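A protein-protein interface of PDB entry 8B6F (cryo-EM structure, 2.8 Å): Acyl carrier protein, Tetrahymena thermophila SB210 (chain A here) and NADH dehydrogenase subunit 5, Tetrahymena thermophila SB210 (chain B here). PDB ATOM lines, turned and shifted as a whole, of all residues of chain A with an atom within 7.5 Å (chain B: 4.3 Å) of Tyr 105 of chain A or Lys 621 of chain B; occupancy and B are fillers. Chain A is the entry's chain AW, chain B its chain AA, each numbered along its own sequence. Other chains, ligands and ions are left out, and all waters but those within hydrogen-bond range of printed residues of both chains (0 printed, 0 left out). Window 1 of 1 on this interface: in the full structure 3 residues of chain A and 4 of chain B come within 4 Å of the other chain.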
ATOM      1  N   ARG A  60     -17.198  -4.472 -13.751  1.00  0.00           N
ATOM      2  CA  ARG A  60     -17.862  -5.013 -14.931  1.00  0.00           C
ATOM      3  C   ARG A  60     -18.029  -6.523 -14.830  1.00  0.00           C
ATOM      4  O   ARG A  60     -19.076  -7.064 -15.198  1.00  0.00           O
ATOM      5  CB  ARG A  60     -17.082  -4.634 -16.188  1.00  0.00           C
ATOM      6  CG  ARG A  60     -17.244  -3.174 -16.577  1.00  0.00           C
ATOM      7  CD  ARG A  60     -16.095  -2.681 -17.436  1.00  0.00           C
ATOM      8  NE  ARG A  60     -15.995  -3.397 -18.701  1.00  0.00           N
ATOM      9  CZ  ARG A  60     -15.069  -3.160 -19.620  1.00  0.00           C
ATOM     10  NH1 ARG A  60     -14.147  -2.229 -19.448  1.00  0.00           N
ATOM     11  NH2 ARG A  60     -15.068  -3.878 -20.739  1.00  0.00           N
ATOM     12  N   LEU A  98     -17.384 -17.040 -21.214  1.00  0.00           N
ATOM     13  CA  LEU A  98     -17.533 -16.683 -22.621  1.00  0.00           C
ATOM     14  C   LEU A  98     -18.088 -15.274 -22.767  1.00  0.00           C
ATOM     15  O   LEU A  98     -17.601 -14.490 -23.589  1.00  0.00           O
ATOM     16  CB  LEU A  98     -18.434 -17.691 -23.332  1.00  0.00           C
ATOM     17  CG  LEU A  98     -17.839 -19.074 -23.602  1.00  0.00           C
ATOM     18  CD1 LEU A  98     -18.902 -20.001 -24.155  1.00  0.00           C
ATOM     19  CD2 LEU A  98     -16.668 -18.981 -24.565  1.00  0.00           C
ATOM     20  N   GLU A  99     -19.111 -14.933 -21.983  1.00  0.00           N
ATOM     21  CA  GLU A  99     -19.653 -13.582 -22.048  1.00  0.00           C
ATOM     22  C   GLU A  99     -18.652 -12.558 -21.531  1.00  0.00           C
ATOM     23  O   GLU A  99     -18.640 -11.415 -21.999  1.00  0.00           O
ATOM     24  CB  GLU A  99     -20.963 -13.497 -21.267  1.00  0.00           C
ATOM     25  CG  GLU A  99     -22.096 -14.304 -21.882  1.00  0.00           C
ATOM     26  CD  GLU A  99     -22.307 -14.001 -23.355  1.00  0.00           C
ATOM     27  OE1 GLU A  99     -22.032 -12.859 -23.776  1.00  0.00           O
ATOM     28  OE2 GLU A  99     -22.741 -14.911 -24.093  1.00  0.00           O
ATOM     29  N   ALA A 100     -17.812 -12.944 -20.570  1.00  0.00           N
ATOM     30  CA  ALA A 100     -16.756 -12.047 -20.114  1.00  0.00           C
ATOM     31  C   ALA A 100     -15.737 -11.800 -21.216  1.00  0.00           C
ATOM     32  O   ALA A 100     -15.269 -10.670 -21.395  1.00  0.00           O
ATOM     33  CB  ALA A 100     -16.074 -12.623 -18.874  1.00  0.00           C
ATOM     34  N   GLU A 101     -15.383 -12.842 -21.969  1.00  0.00           N
ATOM     35  CA  GLU A 101     -14.498 -12.657 -23.113  1.00  0.00           C
ATOM     36  C   GLU A 101     -15.107 -11.684 -24.113  1.00  0.00           C
ATOM     37  O   GLU A 101     -14.426 -10.785 -24.618  1.00  0.00           O
ATOM     38  CB  GLU A 101     -14.224 -14.006 -23.780  1.00  0.00           C
ATOM     39  CG  GLU A 101     -13.363 -14.945 -22.953  1.00  0.00           C
ATOM     40  CD  GLU A 101     -13.214 -16.308 -23.601  1.00  0.00           C
ATOM     41  OE1 GLU A 101     -13.512 -16.427 -24.807  1.00  0.00           O
ATOM     42  OE2 GLU A 101     -12.806 -17.261 -22.905  1.00  0.00           O
ATOM     43  N   ASN A 102     -16.394 -11.854 -24.416  1.00  0.00           N
ATOM     44  CA  ASN A 102     -17.062 -10.939 -25.332  1.00  0.00           C
ATOM     45  C   ASN A 102     -17.055  -9.517 -24.786  1.00  0.00           C
ATOM     46  O   ASN A 102     -16.833  -8.556 -25.531  1.00  0.00           O
ATOM     47  CB  ASN A 102     -18.493 -11.408 -25.584  1.00  0.00           C
ATOM     48  CG  ASN A 102     -18.545 -12.743 -26.296  1.00  0.00           C
ATOM     49  OD1 ASN A 102     -19.077 -13.719 -25.769  1.00  0.00           O
ATOM     50  ND2 ASN A 102     -17.984 -12.796 -27.498  1.00  0.00           N
ATOM     51  N   GLU A 103     -17.298  -9.365 -23.484  1.00  0.00           N
ATOM     52  CA  GLU A 103     -17.359  -8.035 -22.890  1.00  0.00           C
ATOM     53  C   GLU A 103     -15.996  -7.356 -22.906  1.00  0.00           C
ATOM     54  O   GLU A 103     -15.896  -6.160 -23.205  1.00  0.00           O
ATOM     55  CB  GLU A 103     -17.893  -8.138 -21.460  1.00  0.00           C
ATOM     56  CG  GLU A 103     -18.706  -6.937 -21.000  1.00  0.00           C
ATOM     57  CD  GLU A 103     -17.848  -5.744 -20.629  1.00  0.00           C
ATOM     58  OE1 GLU A 103     -16.615  -5.900 -20.532  1.00  0.00           O
ATOM     59  OE2 GLU A 103     -18.411  -4.647 -20.428  1.00  0.00           O
ATOM     60  N   PHE A 104     -14.936  -8.097 -22.587  1.00  0.00           N
ATOM     61  CA  PHE A 104     -13.608  -7.524 -22.420  1.00  0.00           C
ATOM     62  C   PHE A 104     -12.767  -7.550 -23.690  1.00  0.00           C
ATOM     63  O   PHE A 104     -11.638  -7.052 -23.671  1.00  0.00           O
ATOM     64  CB  PHE A 104     -12.858  -8.251 -21.301  1.00  0.00           C
ATOM     65  CG  PHE A 104     -13.406  -7.980 -19.932  1.00  0.00           C
ATOM     66  CD1 PHE A 104     -13.242  -6.738 -19.344  1.00  0.00           C
ATOM     67  CD2 PHE A 104     -14.069  -8.968 -19.226  1.00  0.00           C
ATOM     68  CE1 PHE A 104     -13.739  -6.484 -18.082  1.00  0.00           C
ATOM     69  CE2 PHE A 104     -14.569  -8.721 -17.963  1.00  0.00           C
ATOM     70  CZ  PHE A 104     -14.404  -7.477 -17.391  1.00  0.00           C
ATOM     71  N   TYR A 105     -13.274  -8.116 -24.784  1.00  0.00           N
ATOM     72  CA  TYR A 105     -12.584  -8.064 -26.072  1.00  0.00           C
ATOM     73  C   TYR A 105     -11.282  -8.864 -26.032  1.00  0.00           C
ATOM     74  O   TYR A 105     -10.262  -8.445 -26.577  1.00  0.00           O
ATOM     75  CB  TYR A 105     -12.318  -6.613 -26.489  1.00  0.00           C
ATOM     76  CG  TYR A 105     -11.874  -6.437 -27.927  1.00  0.00           C
ATOM     77  CD1 TYR A 105     -12.786  -6.503 -28.971  1.00  0.00           C
ATOM     78  CD2 TYR A 105     -10.546  -6.178 -28.234  1.00  0.00           C
ATOM     79  CE1 TYR A 105     -12.384  -6.335 -30.283  1.00  0.00           C
ATOM     80  CE2 TYR A 105     -10.135  -6.006 -29.541  1.00  0.00           C
ATOM     81  CZ  TYR A 105     -11.059  -6.085 -30.560  1.00  0.00           C
ATOM     82  OH  TYR A 105     -10.650  -5.915 -31.862  1.00  0.00           O
ATOM     83  N   ILE A 106     -11.313 -10.026 -25.379  1.00  0.00           N
ATOM     84  CA  ILE A 106     -10.151 -10.900 -25.273  1.00  0.00           C
ATOM     85  C   ILE A 106     -10.621 -12.349 -25.312  1.00  0.00           C
ATOM     86  O   ILE A 106     -11.804 -12.648 -25.152  1.00  0.00           O
ATOM     87  CB  ILE A 106      -9.330 -10.636 -23.992  1.00  0.00           C
ATOM     88  CG1 ILE A 106     -10.193 -10.875 -22.749  1.00  0.00           C
ATOM     89  CG2 ILE A 106      -8.778  -9.218 -24.010  1.00  0.00           C
ATOM     90  CD1 ILE A 106      -9.478 -10.636 -21.433  1.00  0.00           C
ATOM     91  N   GLU A 107      -9.669 -13.249 -25.536  1.00  0.00           N
ATOM     92  CA  GLU A 107      -9.902 -14.686 -25.512  1.00  0.00           C
ATOM     93  C   GLU A 107      -9.106 -15.293 -24.369  1.00  0.00           C
ATOM     94  O   GLU A 107      -7.901 -15.051 -24.252  1.00  0.00           O
ATOM     95  CB  GLU A 107      -9.497 -15.334 -26.839  1.00  0.00           C
ATOM     96  CG  GLU A 107     -10.312 -14.869 -28.031  1.00  0.00           C
ATOM     97  CD  GLU A 107     -11.767 -15.271 -27.936  1.00  0.00           C
ATOM     98  OE1 GLU A 107     -12.088 -16.141 -27.103  1.00  0.00           O
ATOM     99  OE2 GLU A 107     -12.589 -14.717 -28.695  1.00  0.00           O
ATOM    100  N   ASN A 129      -3.978  -8.676 -18.487  1.00  0.00           N
ATOM    101  CA  ASN A 129      -3.889  -9.151 -19.859  1.00  0.00           C
ATOM    102  C   ASN A 129      -3.742  -7.979 -20.820  1.00  0.00           C
ATOM    103  O   ASN A 129      -4.484  -6.998 -20.741  1.00  0.00           O
ATOM    104  CB  ASN A 129      -5.127  -9.976 -20.212  1.00  0.00           C
ATOM    105  CG  ASN A 129      -4.999 -10.683 -21.548  1.00  0.00           C
ATOM    106  OD1 ASN A 129      -4.354 -10.188 -22.470  1.00  0.00           O
ATOM    107  ND2 ASN A 129      -5.616 -11.852 -21.655  1.00  0.00           N
ATOM    108  N   PHE A 130      -2.772  -8.085 -21.724  1.00  0.00           N
ATOM    109  CA  PHE A 130      -2.634  -7.156 -22.841  1.00  0.00           C
ATOM    110  C   PHE A 130      -3.645  -7.568 -23.904  1.00  0.00           C
ATOM    111  O   PHE A 130      -3.524  -8.646 -24.496  1.00  0.00           O
ATOM    112  CB  PHE A 130      -1.205  -7.191 -23.375  1.00  0.00           C
ATOM    113  CG  PHE A 130      -0.872  -6.071 -24.319  1.00  0.00           C
ATOM    114  CD1 PHE A 130      -0.469  -4.839 -23.837  1.00  0.00           C
ATOM    115  CD2 PHE A 130      -0.924  -6.262 -25.689  1.00  0.00           C
ATOM    116  CE1 PHE A 130      -0.142  -3.812 -24.701  1.00  0.00           C
ATOM    117  CE2 PHE A 130      -0.599  -5.238 -26.559  1.00  0.00           C
ATOM    118  CZ  PHE A 130      -0.209  -4.011 -26.063  1.00  0.00           C
ATOM    119  N   PHE A 131      -4.647  -6.721 -24.145  1.00  0.00           N
ATOM    120  CA  PHE A 131      -5.783  -7.150 -24.955  1.00  0.00           C
ATOM    121  C   PHE A 131      -5.346  -7.665 -26.320  1.00  0.00           C
ATOM    122  O   PHE A 131      -6.014  -8.530 -26.894  1.00  0.00           O
ATOM    123  CB  PHE A 131      -6.785  -6.004 -25.111  1.00  0.00           C
ATOM    124  CG  PHE A 131      -7.555  -5.683 -23.852  1.00  0.00           C
ATOM    125  CD1 PHE A 131      -7.367  -6.414 -22.685  1.00  0.00           C
ATOM    126  CD2 PHE A 131      -8.478  -4.651 -23.844  1.00  0.00           C
ATOM    127  CE1 PHE A 131      -8.079  -6.116 -21.540  1.00  0.00           C
ATOM    128  CE2 PHE A 131      -9.194  -4.348 -22.702  1.00  0.00           C
ATOM    129  CZ  PHE A 131      -8.993  -5.082 -21.547  1.00  0.00           C
ATOM    130  N   THR A 132      -4.234  -7.162 -26.852  1.00  0.00           N
ATOM    131  CA  THR A 132      -3.688  -7.653 -28.108  1.00  0.00           C
ATOM    132  C   THR A 132      -2.661  -8.760 -27.896  1.00  0.00           C
ATOM    133  O   THR A 132      -1.794  -8.965 -28.752  1.00  0.00           O
ATOM    134  CB  THR A 132      -3.060  -6.499 -28.895  1.00  0.00           C
ATOM    135  OG1 THR A 132      -3.860  -5.319 -28.739  1.00  0.00           O
ATOM    136  CG2 THR A 132      -2.968  -6.840 -30.381  1.00  0.00           C
ATOM    137  N   ARG B 533     -10.714  -2.833 -36.216  1.00  0.00           N
ATOM    138  CA  ARG B 533      -9.542  -3.324 -35.491  1.00  0.00           C
ATOM    139  C   ARG B 533      -8.949  -4.560 -36.172  1.00  0.00           C
ATOM    140  O   ARG B 533      -8.750  -5.600 -35.543  1.00  0.00           O
ATOM    141  CB  ARG B 533      -9.883  -3.629 -34.032  1.00  0.00           C
ATOM    142  CG  ARG B 533     -10.680  -2.551 -33.317  1.00  0.00           C
ATOM    143  CD  ARG B 533      -9.794  -1.472 -32.733  1.00  0.00           C
ATOM    144  NE  ARG B 533     -10.548  -0.597 -31.843  1.00  0.00           N
ATOM    145  CZ  ARG B 533     -10.891  -0.909 -30.601  1.00  0.00           C
ATOM    146  NH1 ARG B 533     -10.567  -2.073 -30.066  1.00  0.00           N
ATOM    147  NH2 ARG B 533     -11.581  -0.032 -29.877  1.00  0.00           N
ATOM    148  N   ARG B 540     -18.283 -10.234 -38.072  1.00  0.00           N
ATOM    149  CA  ARG B 540     -18.164  -9.382 -36.897  1.00  0.00           C
ATOM    150  C   ARG B 540     -18.408  -7.913 -37.218  1.00  0.00           C
ATOM    151  O   ARG B 540     -18.072  -7.048 -36.404  1.00  0.00           O
ATOM    152  CB  ARG B 540     -16.785  -9.547 -36.260  1.00  0.00           C
ATOM    153  CG  ARG B 540     -16.612 -10.837 -35.486  1.00  0.00           C
ATOM    154  CD  ARG B 540     -15.261 -10.881 -34.798  1.00  0.00           C
ATOM    155  NE  ARG B 540     -15.107 -12.067 -33.966  1.00  0.00           N
ATOM    156  CZ  ARG B 540     -14.029 -12.342 -33.246  1.00  0.00           C
ATOM    157  NH1 ARG B 540     -12.982 -11.533 -33.231  1.00  0.00           N
ATOM    158  NH2 ARG B 540     -13.998 -13.458 -32.523  1.00  0.00           N
ATOM    159  N   LYS B 619     -23.125  -7.215 -35.229  1.00  0.00           N
ATOM    160  CA  LYS B 619     -22.505  -8.483 -34.873  1.00  0.00           C
ATOM    161  C   LYS B 619     -21.140  -8.328 -34.219  1.00  0.00           C
ATOM    162  O   LYS B 619     -20.642  -9.295 -33.632  1.00  0.00           O
ATOM    163  CB  LYS B 619     -22.354  -9.365 -36.121  1.00  0.00           C
ATOM    164  CG  LYS B 619     -23.675  -9.743 -36.774  1.00  0.00           C
ATOM    165  CD  LYS B 619     -23.472 -10.463 -38.100  1.00  0.00           C
ATOM    166  CE  LYS B 619     -22.917  -9.528 -39.165  1.00  0.00           C
ATOM    167  NZ  LYS B 619     -22.851 -10.176 -40.504  1.00  0.00           N
ATOM    168  N   GLY B 620     -20.530  -7.154 -34.294  1.00  0.00           N
ATOM    169  CA  GLY B 620     -19.194  -6.967 -33.772  1.00  0.00           C
ATOM    170  C   GLY B 620     -19.163  -6.894 -32.259  1.00  0.00           C
ATOM    171  O   GLY B 620     -20.185  -6.855 -31.575  1.00  0.00           O
ATOM    172  N   LYS B 621     -17.942  -6.870 -31.732  1.00  0.00           N
ATOM    173  CA  LYS B 621     -17.752  -6.803 -30.290  1.00  0.00           C
ATOM    174  C   LYS B 621     -18.311  -5.500 -29.732  1.00  0.00           C
ATOM    175  O   LYS B 621     -18.287  -4.454 -30.383  1.00  0.00           O
ATOM    176  CB  LYS B 621     -16.268  -6.927 -29.941  1.00  0.00           C
ATOM    177  CG  LYS B 621     -15.890  -8.257 -29.308  1.00  0.00           C
ATOM    178  CD  LYS B 621     -16.129  -9.423 -30.251  1.00  0.00           C
ATOM    179  CE  LYS B 621     -15.690 -10.731 -29.612  1.00  0.00           C
ATOM    180  NZ  LYS B 621     -16.022 -11.906 -30.464  1.00  0.00           N
ATOM    181  N   LYS B 622     -18.822  -5.580 -28.503  1.00  0.00           N
ATOM    182  CA  LYS B 622     -19.420  -4.411 -27.868  1.00  0.00           C
ATOM    183  C   LYS B 622     -18.439  -3.252 -27.794  1.00  0.00           C
ATOM    184  O   LYS B 622     -18.846  -2.088 -27.871  1.00  0.00           O
ATOM    185  CB  LYS B 622     -19.910  -4.781 -26.469  1.00  0.00           C
ATOM    186  CG  LYS B 622     -20.726  -3.699 -25.791  1.00  0.00           C
ATOM    187  CD  LYS B 622     -20.840  -3.934 -24.294  1.00  0.00           C
ATOM    188  CE  LYS B 622     -21.430  -5.298 -23.981  1.00  0.00           C
ATOM    189  NZ  LYS B 622     -21.669  -5.473 -22.522  1.00  0.00           N
ATOM    190  N   ALA B 623     -17.148  -3.546 -27.639  1.00  0.00           N
ATOM    191  CA  ALA B 623     -16.158  -2.484 -27.493  1.00  0.00           C
ATOM    192  C   ALA B 623     -16.096  -1.608 -28.736  1.00  0.00           C
ATOM    193  O   ALA B 623     -15.980  -0.382 -28.635  1.00  0.00           O
ATOM    194  CB  ALA B 623     -14.786  -3.086 -27.195  1.00  0.00           C
ATOM    195  N   ILE B 624     -16.169  -2.217 -29.920  1.00  0.00           N
ATOM    196  CA  ILE B 624     -16.035  -1.449 -31.155  1.00  0.00           C
ATOM    197  C   ILE B 624     -17.046  -0.311 -31.186  1.00  0.00           C
ATOM    198  O   ILE B 624     -16.718   0.822 -31.560  1.00  0.00           O
ATOM    199  CB  ILE B 624     -16.191  -2.370 -32.379  1.00  0.00           C
ATOM    200  CG1 ILE B 624     -15.218  -3.551 -32.310  1.00  0.00           C
ATOM    201  CG2 ILE B 624     -15.973  -1.590 -33.668  1.00  0.00           C
ATOM    202  CD1 ILE B 624     -13.768  -3.165 -32.178  1.00  0.00           C
ATOM    203  N   TYR B 625     -18.289  -0.589 -30.789  1.00  0.00           N
ATOM    204  CA  TYR B 625     -19.328   0.432 -30.827  1.00  0.00           C
ATOM    205  C   TYR B 625     -19.255   1.370 -29.627  1.00  0.00           C
ATOM    206  O   TYR B 625     -19.409   2.586 -29.780  1.00  0.00           O
ATOM    207  CB  TYR B 625     -20.702  -0.232 -30.890  1.00  0.00           C
ATOM    208  CG  TYR B 625     -20.836  -1.235 -32.008  1.00  0.00           C
ATOM    209  CD1 TYR B 625     -21.135  -0.822 -33.298  1.00  0.00           C
ATOM    210  CD2 TYR B 625     -20.668  -2.592 -31.776  1.00  0.00           C
ATOM    211  CE1 TYR B 625     -21.262  -1.727 -34.325  1.00  0.00           C
ATOM    212  CE2 TYR B 625     -20.793  -3.509 -32.800  1.00  0.00           C
ATOM    213  CZ  TYR B 625     -21.091  -3.067 -34.072  1.00  0.00           C
ATOM    214  OH  TYR B 625     -21.219  -3.965 -35.101  1.00  0.00           O
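The side-chain amino group of Lys 622 of chain B is in salt-bridge range of the side-chain carboxylate of Glu 103 of chain A, 3.96 Å away.
The side-chain carboxylate (OE1) of Glu 103 of chain A lies within salt-bridge range of the guanidinium group (NH2) of Arg 60 of chain A. The backbone carbonyl oxygen of Leu 98 of chain A lies close to the side-chain amide oxygen of Asn 102 of chain A (2.7 Å).
Among the printed residues, pairs that only touch across the chains: Asn 102 of chain A with Lys 621 of chain B, Tyr 105 of chain A with Arg 533 of chain B, Tyr 105 of chain A with Lys 621 of chain B and Tyr 105 of chain A with Ile 624 of chain B.
Printed residues of chain B within 4 Å of Asn 102 of chain A: Lys 621 (3.7 Å). Of the printed residues of chain B, Glu 103 of chain A touches Lys 622. Phe 130 of chain A touches none of the printed residues of chain B. Of the printed residues of chain A, Arg 533 of chain B touches Tyr 105 (3.2 Å). Of chain A, only Asn 102 and Tyr 105 come within 4 Å of Lys 621 of chain B. Of the printed residues of chain A, Lys 622 of chain B touches Glu 103 (3.6 Å).
Of the 9 printed residues of chain B, 4 touch a printed residue of chain A. Of the 15 printed residues of chain A, 3 touch a printed residue of chain B. Hydrophobic or aromatic side chains of chain A that line the printed part of chain B: Tyr 105. Among the printed residues, 5 pairs touch across the chains. Among the printed residues, Asp or Glu carboxylates within 4 Å of a Lys or Arg side-chain nitrogen of the other chain: Glu 103 of chain A with Lys 622 of chain B (3.96 Å).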
